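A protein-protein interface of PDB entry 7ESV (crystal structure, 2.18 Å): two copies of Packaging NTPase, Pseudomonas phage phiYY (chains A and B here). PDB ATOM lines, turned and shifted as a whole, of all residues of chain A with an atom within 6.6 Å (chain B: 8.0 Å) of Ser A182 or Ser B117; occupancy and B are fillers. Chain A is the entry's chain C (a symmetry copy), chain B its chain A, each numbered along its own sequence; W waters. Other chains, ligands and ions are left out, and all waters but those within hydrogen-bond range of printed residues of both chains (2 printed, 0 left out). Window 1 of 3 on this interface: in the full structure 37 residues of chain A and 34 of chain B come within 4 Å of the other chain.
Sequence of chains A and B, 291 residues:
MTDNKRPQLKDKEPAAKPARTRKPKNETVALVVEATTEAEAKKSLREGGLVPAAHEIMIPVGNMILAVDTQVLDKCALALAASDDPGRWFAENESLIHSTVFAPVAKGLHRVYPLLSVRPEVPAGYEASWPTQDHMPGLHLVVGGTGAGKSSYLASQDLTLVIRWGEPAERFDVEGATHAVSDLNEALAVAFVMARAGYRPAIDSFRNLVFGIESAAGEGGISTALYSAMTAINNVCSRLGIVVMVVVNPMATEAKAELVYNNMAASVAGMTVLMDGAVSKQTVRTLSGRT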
ATOM      1  N   ARG A  20      -8.479 -17.026  26.378  1.00  0.00           N
ATOM      2  CA  ARG A  20      -8.056 -18.402  26.169  1.00  0.00           C
ATOM      3  C   ARG A  20      -6.738 -18.643  26.889  1.00  0.00           C
ATOM      4  O   ARG A  20      -5.775 -17.893  26.697  1.00  0.00           O
ATOM      5  CB  ARG A  20      -7.912 -18.704  24.675  1.00  0.00           C
ATOM      6  CG  ARG A  20      -9.235 -18.749  23.924  1.00  0.00           C
ATOM      7  CD  ARG A  20      -9.056 -19.113  22.455  1.00  0.00           C
ATOM      8  NE  ARG A  20     -10.270 -18.837  21.690  1.00  0.00           N
ATOM      9  CZ  ARG A  20     -10.510 -19.295  20.466  1.00  0.00           C
ATOM     10  NH1 ARG A  20      -9.618 -20.060  19.852  1.00  0.00           N
ATOM     11  NH2 ARG A  20     -11.647 -18.987  19.854  1.00  0.00           N
ATOM     12  N   ARG A 164     -14.903 -21.913  12.988  1.00  0.00           N
ATOM     13  CA  ARG A 164     -14.776 -20.804  12.054  1.00  0.00           C
ATOM     14  C   ARG A 164     -13.308 -20.491  11.813  1.00  0.00           C
ATOM     15  O   ARG A 164     -12.549 -20.266  12.762  1.00  0.00           O
ATOM     16  CB  ARG A 164     -15.509 -19.568  12.573  1.00  0.00           C
ATOM     17  CG  ARG A 164     -17.011 -19.739  12.604  1.00  0.00           C
ATOM     18  CD  ARG A 164     -17.639 -19.391  11.273  1.00  0.00           C
ATOM     19  NE  ARG A 164     -17.562 -17.961  10.999  1.00  0.00           N
ATOM     20  CZ  ARG A 164     -17.570 -17.436   9.779  1.00  0.00           C
ATOM     21  NH1 ARG A 164     -17.652 -18.227   8.718  1.00  0.00           N
ATOM     22  NH2 ARG A 164     -17.496 -16.122   9.620  1.00  0.00           N
ATOM     23  N   TRP A 165     -12.914 -20.470  10.541  1.00  0.00           N
ATOM     24  CA  TRP A 165     -11.516 -20.293  10.173  1.00  0.00           C
ATOM     25  C   TRP A 165     -11.419 -19.640   8.804  1.00  0.00           C
ATOM     26  O   TRP A 165     -12.046 -20.104   7.847  1.00  0.00           O
ATOM     27  CB  TRP A 165     -10.778 -21.635  10.165  1.00  0.00           C
ATOM     28  CG  TRP A 165      -9.354 -21.514   9.733  1.00  0.00           C
ATOM     29  CD1 TRP A 165      -8.443 -20.596  10.165  1.00  0.00           C
ATOM     30  CD2 TRP A 165      -8.679 -22.328   8.768  1.00  0.00           C
ATOM     31  NE1 TRP A 165      -7.238 -20.794   9.536  1.00  0.00           N
ATOM     32  CE2 TRP A 165      -7.356 -21.850   8.673  1.00  0.00           C
ATOM     33  CE3 TRP A 165      -9.061 -23.417   7.980  1.00  0.00           C
ATOM     34  CZ2 TRP A 165      -6.417 -22.423   7.822  1.00  0.00           C
ATOM     35  CZ3 TRP A 165      -8.127 -23.984   7.134  1.00  0.00           C
ATOM     36  CH2 TRP A 165      -6.821 -23.487   7.062  1.00  0.00           C
ATOM     37  N   GLY A 166     -10.625 -18.574   8.717  1.00  0.00           N
ATOM     38  CA  GLY A 166     -10.313 -17.952   7.444  1.00  0.00           C
ATOM     39  C   GLY A 166     -11.421 -17.138   6.820  1.00  0.00           C
ATOM     40  O   GLY A 166     -11.286 -16.721   5.667  1.00  0.00           O
ATOM     41  N   GLU A 167     -12.510 -16.894   7.543  1.00  0.00           N
ATOM     42  CA  GLU A 167     -13.661 -16.164   7.041  1.00  0.00           C
ATOM     43  C   GLU A 167     -13.848 -14.870   7.825  1.00  0.00           C
ATOM     44  O   GLU A 167     -13.521 -14.813   9.015  1.00  0.00           O
ATOM     45  CB  GLU A 167     -14.933 -17.015   7.150  1.00  0.00           C
ATOM     46  CG  GLU A 167     -14.926 -18.272   6.291  1.00  0.00           C
ATOM     47  CD  GLU A 167     -15.124 -17.988   4.813  1.00  0.00           C
ATOM     48  OE1 GLU A 167     -15.084 -18.950   4.017  1.00  0.00           O
ATOM     49  OE2 GLU A 167     -15.347 -16.815   4.446  1.00  0.00           O
ATOM     50  N   ALA A 180     -14.034 -19.979  17.034  1.00  0.00           N
ATOM     51  CA  ALA A 180     -13.089 -19.415  16.082  1.00  0.00           C
ATOM     52  C   ALA A 180     -11.690 -19.965  16.324  1.00  0.00           C
ATOM     53  O   ALA A 180     -11.264 -20.141  17.469  1.00  0.00           O
ATOM     54  CB  ALA A 180     -13.079 -17.890  16.185  1.00  0.00           C
ATOM     55  N   VAL A 181     -10.979 -20.251  15.232  1.00  0.00           N
ATOM     56  CA  VAL A 181      -9.582 -20.665  15.277  1.00  0.00           C
ATOM     57  C   VAL A 181      -8.811 -19.858  14.238  1.00  0.00           C
ATOM     58  O   VAL A 181      -9.388 -19.127  13.432  1.00  0.00           O
ATOM     59  CB  VAL A 181      -9.398 -22.180  15.041  1.00  0.00           C
ATOM     60  CG1 VAL A 181     -10.283 -22.988  15.982  1.00  0.00           C
ATOM     61  CG2 VAL A 181      -9.678 -22.535  13.589  1.00  0.00           C
ATOM     62  N   SER A 182      -7.487 -20.009  14.259  1.00  0.00           N
ATOM     63  CA  SER A 182      -6.609 -19.159  13.464  1.00  0.00           C
ATOM     64  C   SER A 182      -5.834 -19.883  12.374  1.00  0.00           C
ATOM     65  O   SER A 182      -5.490 -19.255  11.371  1.00  0.00           O
ATOM     66  CB  SER A 182      -5.608 -18.434  14.374  1.00  0.00           C
ATOM     67  OG  SER A 182      -6.260 -17.844  15.487  1.00  0.00           O
ATOM     68  N   ASP A 183      -5.543 -21.174  12.525  1.00  0.00           N
ATOM     69  CA  ASP A 183      -4.689 -21.864  11.567  1.00  0.00           C
ATOM     70  C   ASP A 183      -5.182 -23.288  11.338  1.00  0.00           C
ATOM     71  O   ASP A 183      -6.060 -23.793  12.043  1.00  0.00           O
ATOM     72  CB  ASP A 183      -3.218 -21.829  12.019  1.00  0.00           C
ATOM     73  CG  ASP A 183      -2.959 -22.633  13.288  1.00  0.00           C
ATOM     74  OD1 ASP A 183      -3.341 -23.818  13.362  1.00  0.00           O
ATOM     75  OD2 ASP A 183      -2.361 -22.064  14.224  1.00  0.00           O
ATOM     76  N   LEU A 184      -4.584 -23.937  10.333  1.00  0.00           N
ATOM     77  CA  LEU A 184      -5.030 -25.265   9.919  1.00  0.00           C
ATOM     78  C   LEU A 184      -4.835 -26.297  11.026  1.00  0.00           C
ATOM     79  O   LEU A 184      -5.660 -27.203  11.182  1.00  0.00           O
ATOM     80  CB  LEU A 184      -4.294 -25.690   8.648  1.00  0.00           C
ATOM     81  CG  LEU A 184      -4.613 -27.070   8.067  1.00  0.00           C
ATOM     82  CD1 LEU A 184      -6.088 -27.173   7.722  1.00  0.00           C
ATOM     83  CD2 LEU A 184      -3.756 -27.347   6.840  1.00  0.00           C
ATOM     84  N   GLU A 186      -5.137 -26.021  14.368  1.00  0.00           N
ATOM     85  CA  GLU A 186      -6.199 -26.016  15.365  1.00  0.00           C
ATOM     86  C   GLU A 186      -7.570 -26.250  14.745  1.00  0.00           C
ATOM     87  O   GLU A 186      -8.462 -26.778  15.417  1.00  0.00           O
ATOM     88  CB  GLU A 186      -6.181 -24.706  16.154  1.00  0.00           C
ATOM     89  CG  GLU A 186      -6.098 -23.449  15.314  1.00  0.00           C
ATOM     90  CD  GLU A 186      -5.868 -22.214  16.161  1.00  0.00           C
ATOM     91  OE1 GLU A 186      -6.600 -22.033  17.158  1.00  0.00           O
ATOM     92  OE2 GLU A 186      -4.966 -21.417  15.826  1.00  0.00           O
ATOM     93  N   ALA A 187      -7.760 -25.870  13.479  1.00  0.00           N
ATOM     94  CA  ALA A 187      -8.987 -26.240  12.782  1.00  0.00           C
ATOM     95  C   ALA A 187      -9.159 -27.753  12.763  1.00  0.00           C
ATOM     96  O   ALA A 187     -10.219 -28.278  13.120  1.00  0.00           O
ATOM     97  CB  ALA A 187      -8.975 -25.679  11.358  1.00  0.00           C
ATOM     98  N   ASN A 208      -8.680 -20.890   3.169  1.00  0.00           N
ATOM     99  CA  ASN A 208      -7.244 -20.631   3.130  1.00  0.00           C
ATOM    100  C   ASN A 208      -6.444 -21.769   2.498  1.00  0.00           C
ATOM    101  O   ASN A 208      -5.354 -21.517   1.974  1.00  0.00           O
ATOM    102  CB  ASN A 208      -6.723 -20.312   4.534  1.00  0.00           C
ATOM    103  CG  ASN A 208      -6.792 -18.821   4.853  1.00  0.00           C
ATOM    104  OD1 ASN A 208      -7.322 -18.032   4.068  1.00  0.00           O
ATOM    105  ND2 ASN A 208      -6.249 -18.433   6.000  1.00  0.00           N
ATOM    106  N   ILE B  57      -1.295 -10.681  18.852  1.00  0.00           N
ATOM    107  CA  ILE B  57      -2.109 -11.243  17.781  1.00  0.00           C
ATOM    108  C   ILE B  57      -1.291 -11.199  16.501  1.00  0.00           C
ATOM    109  O   ILE B  57      -0.863 -10.121  16.069  1.00  0.00           O
ATOM    110  CB  ILE B  57      -3.439 -10.493  17.606  1.00  0.00           C
ATOM    111  CG1 ILE B  57      -4.180 -10.388  18.939  1.00  0.00           C
ATOM    112  CG2 ILE B  57      -4.300 -11.183  16.560  1.00  0.00           C
ATOM    113  CD1 ILE B  57      -5.509  -9.668  18.844  1.00  0.00           C
ATOM    114  N   MET B  58      -1.072 -12.364  15.897  1.00  0.00           N
ATOM    115  CA  MET B  58      -0.334 -12.443  14.647  1.00  0.00           C
ATOM    116  C   MET B  58      -1.212 -12.006  13.482  1.00  0.00           C
ATOM    117  O   MET B  58      -2.410 -12.304  13.441  1.00  0.00           O
ATOM    118  CB  MET B  58       0.180 -13.864  14.416  1.00  0.00           C
ATOM    119  CG  MET B  58       1.473 -14.169  15.151  1.00  0.00           C
ATOM    120  SD  MET B  58       2.042 -15.868  14.957  1.00  0.00           S
ATOM    121  CE  MET B  58       0.537 -16.766  15.322  1.00  0.00           C
ATOM    122  N   ILE B  59      -0.610 -11.288  12.539  1.00  0.00           N
ATOM    123  CA  ILE B  59      -1.322 -10.813  11.355  1.00  0.00           C
ATOM    124  C   ILE B  59      -0.605 -11.311  10.108  1.00  0.00           C
ATOM    125  O   ILE B  59       0.413 -10.725   9.706  1.00  0.00           O
ATOM    126  CB  ILE B  59      -1.435  -9.279  11.345  1.00  0.00           C
ATOM    127  CG1 ILE B  59      -1.892  -8.768  12.713  1.00  0.00           C
ATOM    128  CG2 ILE B  59      -2.386  -8.825  10.246  1.00  0.00           C
ATOM    129  CD1 ILE B  59      -1.969  -7.261  12.806  1.00  0.00           C
ATOM    130  N   PRO B  60      -1.085 -12.376   9.464  1.00  0.00           N
ATOM    131  CA  PRO B  60      -0.441 -12.844   8.229  1.00  0.00           C
ATOM    132  C   PRO B  60      -0.888 -12.007   7.039  1.00  0.00           C
ATOM    133  O   PRO B  60      -2.082 -11.771   6.839  1.00  0.00           O
ATOM    134  CB  PRO B  60      -0.916 -14.295   8.115  1.00  0.00           C
ATOM    135  CG  PRO B  60      -2.266 -14.276   8.758  1.00  0.00           C
ATOM    136  CD  PRO B  60      -2.207 -13.242   9.865  1.00  0.00           C
ATOM    137  N   TYR B 113       2.551 -22.194  12.216  1.00  0.00           N
ATOM    138  CA  TYR B 113       1.159 -21.758  12.116  1.00  0.00           C
ATOM    139  C   TYR B 113       0.725 -21.843  10.657  1.00  0.00           C
ATOM    140  O   TYR B 113       0.687 -20.830   9.942  1.00  0.00           O
ATOM    141  CB  TYR B 113       0.992 -20.358  12.699  1.00  0.00           C
ATOM    142  CG  TYR B 113       1.416 -20.304  14.149  1.00  0.00           C
ATOM    143  CD1 TYR B 113       0.620 -20.860  15.142  1.00  0.00           C
ATOM    144  CD2 TYR B 113       2.624 -19.730  14.523  1.00  0.00           C
ATOM    145  CE1 TYR B 113       1.005 -20.829  16.466  1.00  0.00           C
ATOM    146  CE2 TYR B 113       3.017 -19.692  15.846  1.00  0.00           C
ATOM    147  CZ  TYR B 113       2.204 -20.245  16.812  1.00  0.00           C
ATOM    148  OH  TYR B 113       2.590 -20.215  18.130  1.00  0.00           O
ATOM    149  N   PRO B 114       0.367 -23.040  10.192  1.00  0.00           N
ATOM    150  CA  PRO B 114       0.122 -23.246   8.757  1.00  0.00           C
ATOM    151  C   PRO B 114      -1.158 -22.563   8.298  1.00  0.00           C
ATOM    152  O   PRO B 114      -2.200 -22.659   8.952  1.00  0.00           O
ATOM    153  CB  PRO B 114       0.018 -24.769   8.634  1.00  0.00           C
ATOM    154  CG  PRO B 114      -0.433 -25.221   9.986  1.00  0.00           C
ATOM    155  CD  PRO B 114       0.178 -24.271  10.974  1.00  0.00           C
ATOM    156  N   LEU B 115      -1.068 -21.885   7.151  1.00  0.00           N
ATOM    157  CA  LEU B 115      -2.203 -21.196   6.538  1.00  0.00           C
ATOM    158  C   LEU B 115      -2.849 -20.226   7.522  1.00  0.00           C
ATOM    159  O   LEU B 115      -4.072 -20.090   7.583  1.00  0.00           O
ATOM    160  CB  LEU B 115      -3.221 -22.195   5.991  1.00  0.00           C
ATOM    161  CG  LEU B 115      -2.592 -23.083   4.916  1.00  0.00           C
ATOM    162  CD1 LEU B 115      -3.604 -24.049   4.329  1.00  0.00           C
ATOM    163  CD2 LEU B 115      -1.961 -22.223   3.829  1.00  0.00           C
ATOM    164  N   LEU B 116      -1.999 -19.546   8.291  1.00  0.00           N
ATOM    165  CA  LEU B 116      -2.443 -18.670   9.365  1.00  0.00           C
ATOM    166  C   LEU B 116      -3.468 -17.655   8.882  1.00  0.00           C
ATOM    167  O   LEU B 116      -3.323 -17.059   7.813  1.00  0.00           O
ATOM    168  CB  LEU B 116      -1.239 -17.944   9.963  1.00  0.00           C
ATOM    169  CG  LEU B 116      -1.498 -17.130  11.231  1.00  0.00           C
ATOM    170  CD1 LEU B 116      -2.304 -17.932  12.245  1.00  0.00           C
ATOM    171  CD2 LEU B 116      -0.184 -16.654  11.822  1.00  0.00           C
ATOM    172  N   SER B 117      -4.517 -17.481   9.683  1.00  0.00           N
ATOM    173  CA  SER B 117      -5.460 -16.383   9.529  1.00  0.00           C
ATOM    174  C   SER B 117      -5.529 -15.633  10.850  1.00  0.00           C
ATOM    175  O   SER B 117      -4.638 -15.773  11.694  1.00  0.00           O
ATOM    176  CB  SER B 117      -6.840 -16.900   9.121  1.00  0.00           C
ATOM    177  OG  SER B 117      -7.733 -15.832   8.852  1.00  0.00           O
ATOM    178  N   VAL B 118      -6.569 -14.833  11.043  1.00  0.00           N
ATOM    179  CA  VAL B 118      -6.915 -14.297  12.352  1.00  0.00           C
ATOM    180  C   VAL B 118      -8.323 -14.775  12.672  1.00  0.00           C
ATOM    181  O   VAL B 118      -9.183 -14.826  11.787  1.00  0.00           O
ATOM    182  CB  VAL B 118      -6.817 -12.757  12.400  1.00  0.00           C
ATOM    183  CG1 VAL B 118      -7.141 -12.245  13.797  1.00  0.00           C
ATOM    184  CG2 VAL B 118      -5.428 -12.304  11.978  1.00  0.00           C
ATOM    185  N   ARG B 119      -8.551 -15.152  13.924  1.00  0.00           N
ATOM    186  CA  ARG B 119      -9.823 -15.811  14.176  1.00  0.00           C
ATOM    187  C   ARG B 119     -10.954 -14.788  14.273  1.00  0.00           C
ATOM    188  O   ARG B 119     -10.773 -13.709  14.846  1.00  0.00           O
ATOM    189  CB  ARG B 119      -9.765 -16.649  15.451  1.00  0.00           C
ATOM    190  CG  ARG B 119      -9.412 -15.888  16.714  1.00  0.00           C
ATOM    191  CD  ARG B 119      -9.373 -16.839  17.898  1.00  0.00           C
ATOM    192  NE  ARG B 119      -9.500 -16.146  19.175  1.00  0.00           N
ATOM    193  CZ  ARG B 119      -8.659 -16.305  20.191  1.00  0.00           C
ATOM    194  NH1 ARG B 119      -7.631 -17.135  20.076  1.00  0.00           N
ATOM    195  NH2 ARG B 119      -8.845 -15.639  21.322  1.00  0.00           N
ATOM    196  N   PRO B 120     -12.124 -15.102  13.713  1.00  0.00           N
ATOM    197  CA  PRO B 120     -13.255 -14.164  13.768  1.00  0.00           C
ATOM    198  C   PRO B 120     -13.911 -14.103  15.139  1.00  0.00           C
ATOM    199  O   PRO B 120     -14.647 -15.018  15.525  1.00  0.00           O
ATOM    200  CB  PRO B 120     -14.219 -14.712  12.710  1.00  0.00           C
ATOM    201  CG  PRO B 120     -13.864 -16.156  12.558  1.00  0.00           C
ATOM    202  CD  PRO B 120     -12.427 -16.324  12.947  1.00  0.00           C
ATOM    203  N   SER B 228      -7.227 -13.040   1.305  1.00  0.00           N
ATOM    204  CA  SER B 228      -6.998 -13.543   2.655  1.00  0.00           C
ATOM    205  C   SER B 228      -6.255 -12.526   3.508  1.00  0.00           C
ATOM    206  O   SER B 228      -6.460 -12.473   4.727  1.00  0.00           O
ATOM    207  CB  SER B 228      -6.226 -14.863   2.613  1.00  0.00           C
ATOM    208  OG  SER B 228      -5.010 -14.739   1.897  1.00  0.00           O
ATOM    209  N   ALA B 229      -5.388 -11.718   2.891  1.00  0.00           N
ATOM    210  CA  ALA B 229      -4.713 -10.655   3.627  1.00  0.00           C
ATOM    211  C   ALA B 229      -5.724  -9.696   4.225  1.00  0.00           C
ATOM    212  O   ALA B 229      -5.610  -9.288   5.387  1.00  0.00           O
ATOM    213  CB  ALA B 229      -3.757  -9.893   2.710  1.00  0.00           C
ATOM    214  N   MET B 230      -6.729  -9.322   3.432  1.00  0.00           N
ATOM    215  CA  MET B 230      -7.715  -8.382   3.934  1.00  0.00           C
ATOM    216  C   MET B 230      -8.617  -9.038   4.960  1.00  0.00           C
ATOM    217  O   MET B 230      -9.028  -8.386   5.924  1.00  0.00           O
ATOM    218  CB  MET B 230      -8.547  -7.802   2.805  1.00  0.00           C
ATOM    219  CG  MET B 230      -7.797  -6.946   1.850  1.00  0.00           C
ATOM    220  SD  MET B 230      -9.050  -6.193   0.794  1.00  0.00           S
ATOM    221  CE  MET B 230      -9.747  -7.565  -0.170  1.00  0.00           C
ATOM    222  N   THR B 231      -8.925 -10.327   4.779  1.00  0.00           N
ATOM    223  CA  THR B 231      -9.669 -11.063   5.798  1.00  0.00           C
ATOM    224  C   THR B 231      -8.894 -11.121   7.108  1.00  0.00           C
ATOM    225  O   THR B 231      -9.475 -10.977   8.190  1.00  0.00           O
ATOM    226  CB  THR B 231      -9.986 -12.480   5.313  1.00  0.00           C
ATOM    227  OG1 THR B 231     -10.683 -12.430   4.060  1.00  0.00           O
ATOM    228  CG2 THR B 231     -10.840 -13.212   6.335  1.00  0.00           C
ATOM    229  N   ALA B 232      -7.576 -11.327   7.030  1.00  0.00           N
ATOM    230  CA  ALA B 232      -6.755 -11.355   8.237  1.00  0.00           C
ATOM    231  C   ALA B 232      -6.732  -9.992   8.914  1.00  0.00           C
ATOM    232  O   ALA B 232      -6.956  -9.888  10.126  1.00  0.00           O
ATOM    233  CB  ALA B 232      -5.336 -11.815   7.900  1.00  0.00           C
ATOM    234  N   ILE B 233      -6.461  -8.934   8.146  1.00  0.00           N
ATOM    235  CA  ILE B 233      -6.520  -7.580   8.690  1.00  0.00           C
ATOM    236  C   ILE B 233      -7.936  -7.256   9.154  1.00  0.00           C
ATOM    237  O   ILE B 233      -8.134  -6.572  10.164  1.00  0.00           O
ATOM    238  CB  ILE B 233      -6.020  -6.562   7.647  1.00  0.00           C
ATOM    239  CG1 ILE B 233      -4.538  -6.786   7.337  1.00  0.00           C
ATOM    240  CG2 ILE B 233      -6.253  -5.133   8.129  1.00  0.00           C
ATOM    241  CD1 ILE B 233      -4.052  -6.024   6.120  1.00  0.00           C
ATOM    242  N   ASN B 235     -10.078  -9.383  10.427  1.00  0.00           N
ATOM    243  CA  ASN B 235     -10.417 -10.115  11.638  1.00  0.00           C
ATOM    244  C   ASN B 235      -9.627  -9.659  12.859  1.00  0.00           C
ATOM    245  O   ASN B 235     -10.096  -9.861  13.984  1.00  0.00           O
ATOM    246  CB  ASN B 235     -10.230 -11.615  11.413  1.00  0.00           C
ATOM    247  CG  ASN B 235     -11.434 -12.250  10.744  1.00  0.00           C
ATOM    248  OD1 ASN B 235     -12.463 -11.600  10.552  1.00  0.00           O
ATOM    249  ND2 ASN B 235     -11.317 -13.524  10.393  1.00  0.00           N
ATOM    250  N   VAL B 236      -8.453  -9.048  12.680  1.00  0.00           N
ATOM    251  CA  VAL B 236      -7.801  -8.435  13.832  1.00  0.00           C
ATOM    252  C   VAL B 236      -8.579  -7.202  14.275  1.00  0.00           C
ATOM    253  O   VAL B 236      -8.713  -6.936  15.474  1.00  0.00           O
ATOM    254  CB  VAL B 236      -6.320  -8.110  13.542  1.00  0.00           C
ATOM    255  CG1 VAL B 236      -6.173  -7.158  12.378  1.00  0.00           C
ATOM    256  CG2 VAL B 236      -5.658  -7.518  14.783  1.00  0.00           C
ATOM    257  N   ARG B 239     -11.382  -8.565  16.295  1.00  0.00           N
ATOM    258  CA  ARG B 239     -10.886  -8.920  17.620  1.00  0.00           C
ATOM    259  C   ARG B 239     -10.677  -7.674  18.472  1.00  0.00           C
ATOM    260  O   ARG B 239     -11.022  -7.658  19.659  1.00  0.00           O
ATOM    261  CB  ARG B 239      -9.587  -9.718  17.493  1.00  0.00           C
ATOM    262  CG  ARG B 239      -9.800 -11.171  17.085  1.00  0.00           C
ATOM    263  CD  ARG B 239      -8.534 -12.011  17.221  1.00  0.00           C
ATOM    264  NE  ARG B 239      -8.284 -12.437  18.595  1.00  0.00           N
ATOM    265  CZ  ARG B 239      -7.191 -13.083  18.989  1.00  0.00           C
ATOM    266  NH1 ARG B 239      -7.045 -13.432  20.259  1.00  0.00           N
ATOM    267  NH2 ARG B 239      -6.246 -13.389  18.110  1.00  0.00           N
HETATM  268  O   HOH W   1      -9.329 -17.586  11.327  1.00  0.00           O
HETATM  269  O   HOH W   2      -6.092 -15.032  15.605  1.00  0.00           O
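The backbone carbonyl oxygen (O) of Pro B114 is in hydrogen-bond range of the backbone NH (N) of Leu A184 (3.0 Å). O of Leu B115 lies within hydrogen-bond range of ND2 of Asn A208 (3.2 Å). N of Ser B117 lies within hydrogen-bond range of O of Ser A182 (2.6 Å). O of Glu A167 sits at hydrogen-bond distance from ND2 of Asn B235 (2.9 Å).
O of Val B118 lies within hydrogen-bond range of ND2 of Asn B235, at 2.9 Å. NH2 of Arg A20 sits at hydrogen-bond distance from O of Ala A180 (2.7 Å). The backbone carbonyl oxygen (O) of Arg A164 sits at hydrogen-bond distance from the backbone NH (N) of Val A181. The backbone carbonyl oxygen of Ser A182 lies within hydrogen-bond range of the indole nitrogen of Trp A165 (3.0 Å). The backbone NH (N) of Ser A182 lies within hydrogen-bond range of the side-chain carboxylate (OE2) of Glu A186, 3.3 Å away. The side-chain carboxylate (OD1) of Asp A183 sits at hydrogen-bond distance from the backbone NH (N) of Glu A186, at 3.0 Å.
Among the printed residues, pairs that only touch across the chains: Arg A20 with Arg B119, Arg A164 with Pro B120, Trp A165 with Leu B115, Trp A165 with Ser B117, Gly A166 with Ser B117, Gly A166 with Thr B231, Glu A167 with Pro B120, Glu A167 with Thr B231, Ala A180 with Arg B119, Ala A180 with Pro B120, Val A181 with Arg B119, Ser A182 with Leu B116, Ser A182 with Arg B119, Asp A183 with Tyr B113, Asp A183 with Pro B114, Asn A208 with Leu B116, Asn A208 with Ser B117 and Asn A208 with Ser B228.
Printed residues of chain B within 4 Å of Ser A182: Leu B116, Ser B117 and Arg B119. Ser B117 touches just these residues of chain A: Trp A165 (3.9 Å), Gly A166 (3.6 Å), Ser A182 (2.6 Å) and Asn A208 (3.5 Å). Of the printed residues of chain B, Ala A180 touches Arg B119 (3.6 Å) and Pro B120 (3.3 Å). Of the printed residues of chain B, Asn A208 touches Leu B115 (3.2 Å), Leu B116 (3.7 Å), Ser B117 (3.5 Å) and Ser B228 (3.7 Å). Printed residues of chain A within 4 Å of Asn B235: Glu A167 (2.9 Å). Of the printed residues of chain A, Tyr B113 touches Asp A183 (3.3 Å). The nearest printed residue of chain A that does not touch Thr B231 is Asn A208 (6.3 Å).
Of the 21 printed residues of chain B, 10 touch a printed residue of chain A. Among the printed residues, no Asp or Glu carboxylate lies within 4 Å of a Lys or Arg side-chain nitrogen of the other chain.
No position is printed for both chains. Of the 22 pairs that touch across the chains among the printed residues, none has its exchanged pair printed and touching as well.
Water W1 lies within hydrogen-bond range of the backbone carbonyl oxygen (O) of Val A181 (2.6 Å), the backbone carbonyl oxygen (O) of Val B118 (2.8 Å), the backbone NH (N) of Gly A166 (3.1 Å) and the side-chain hydroxyl (OG) of Ser B117 (3.4 Å). Water W2 lies within hydrogen-bond range of the side-chain hydroxyl of Ser A182, the backbone NH of Arg B119 and the guanidinium group of Arg B239.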
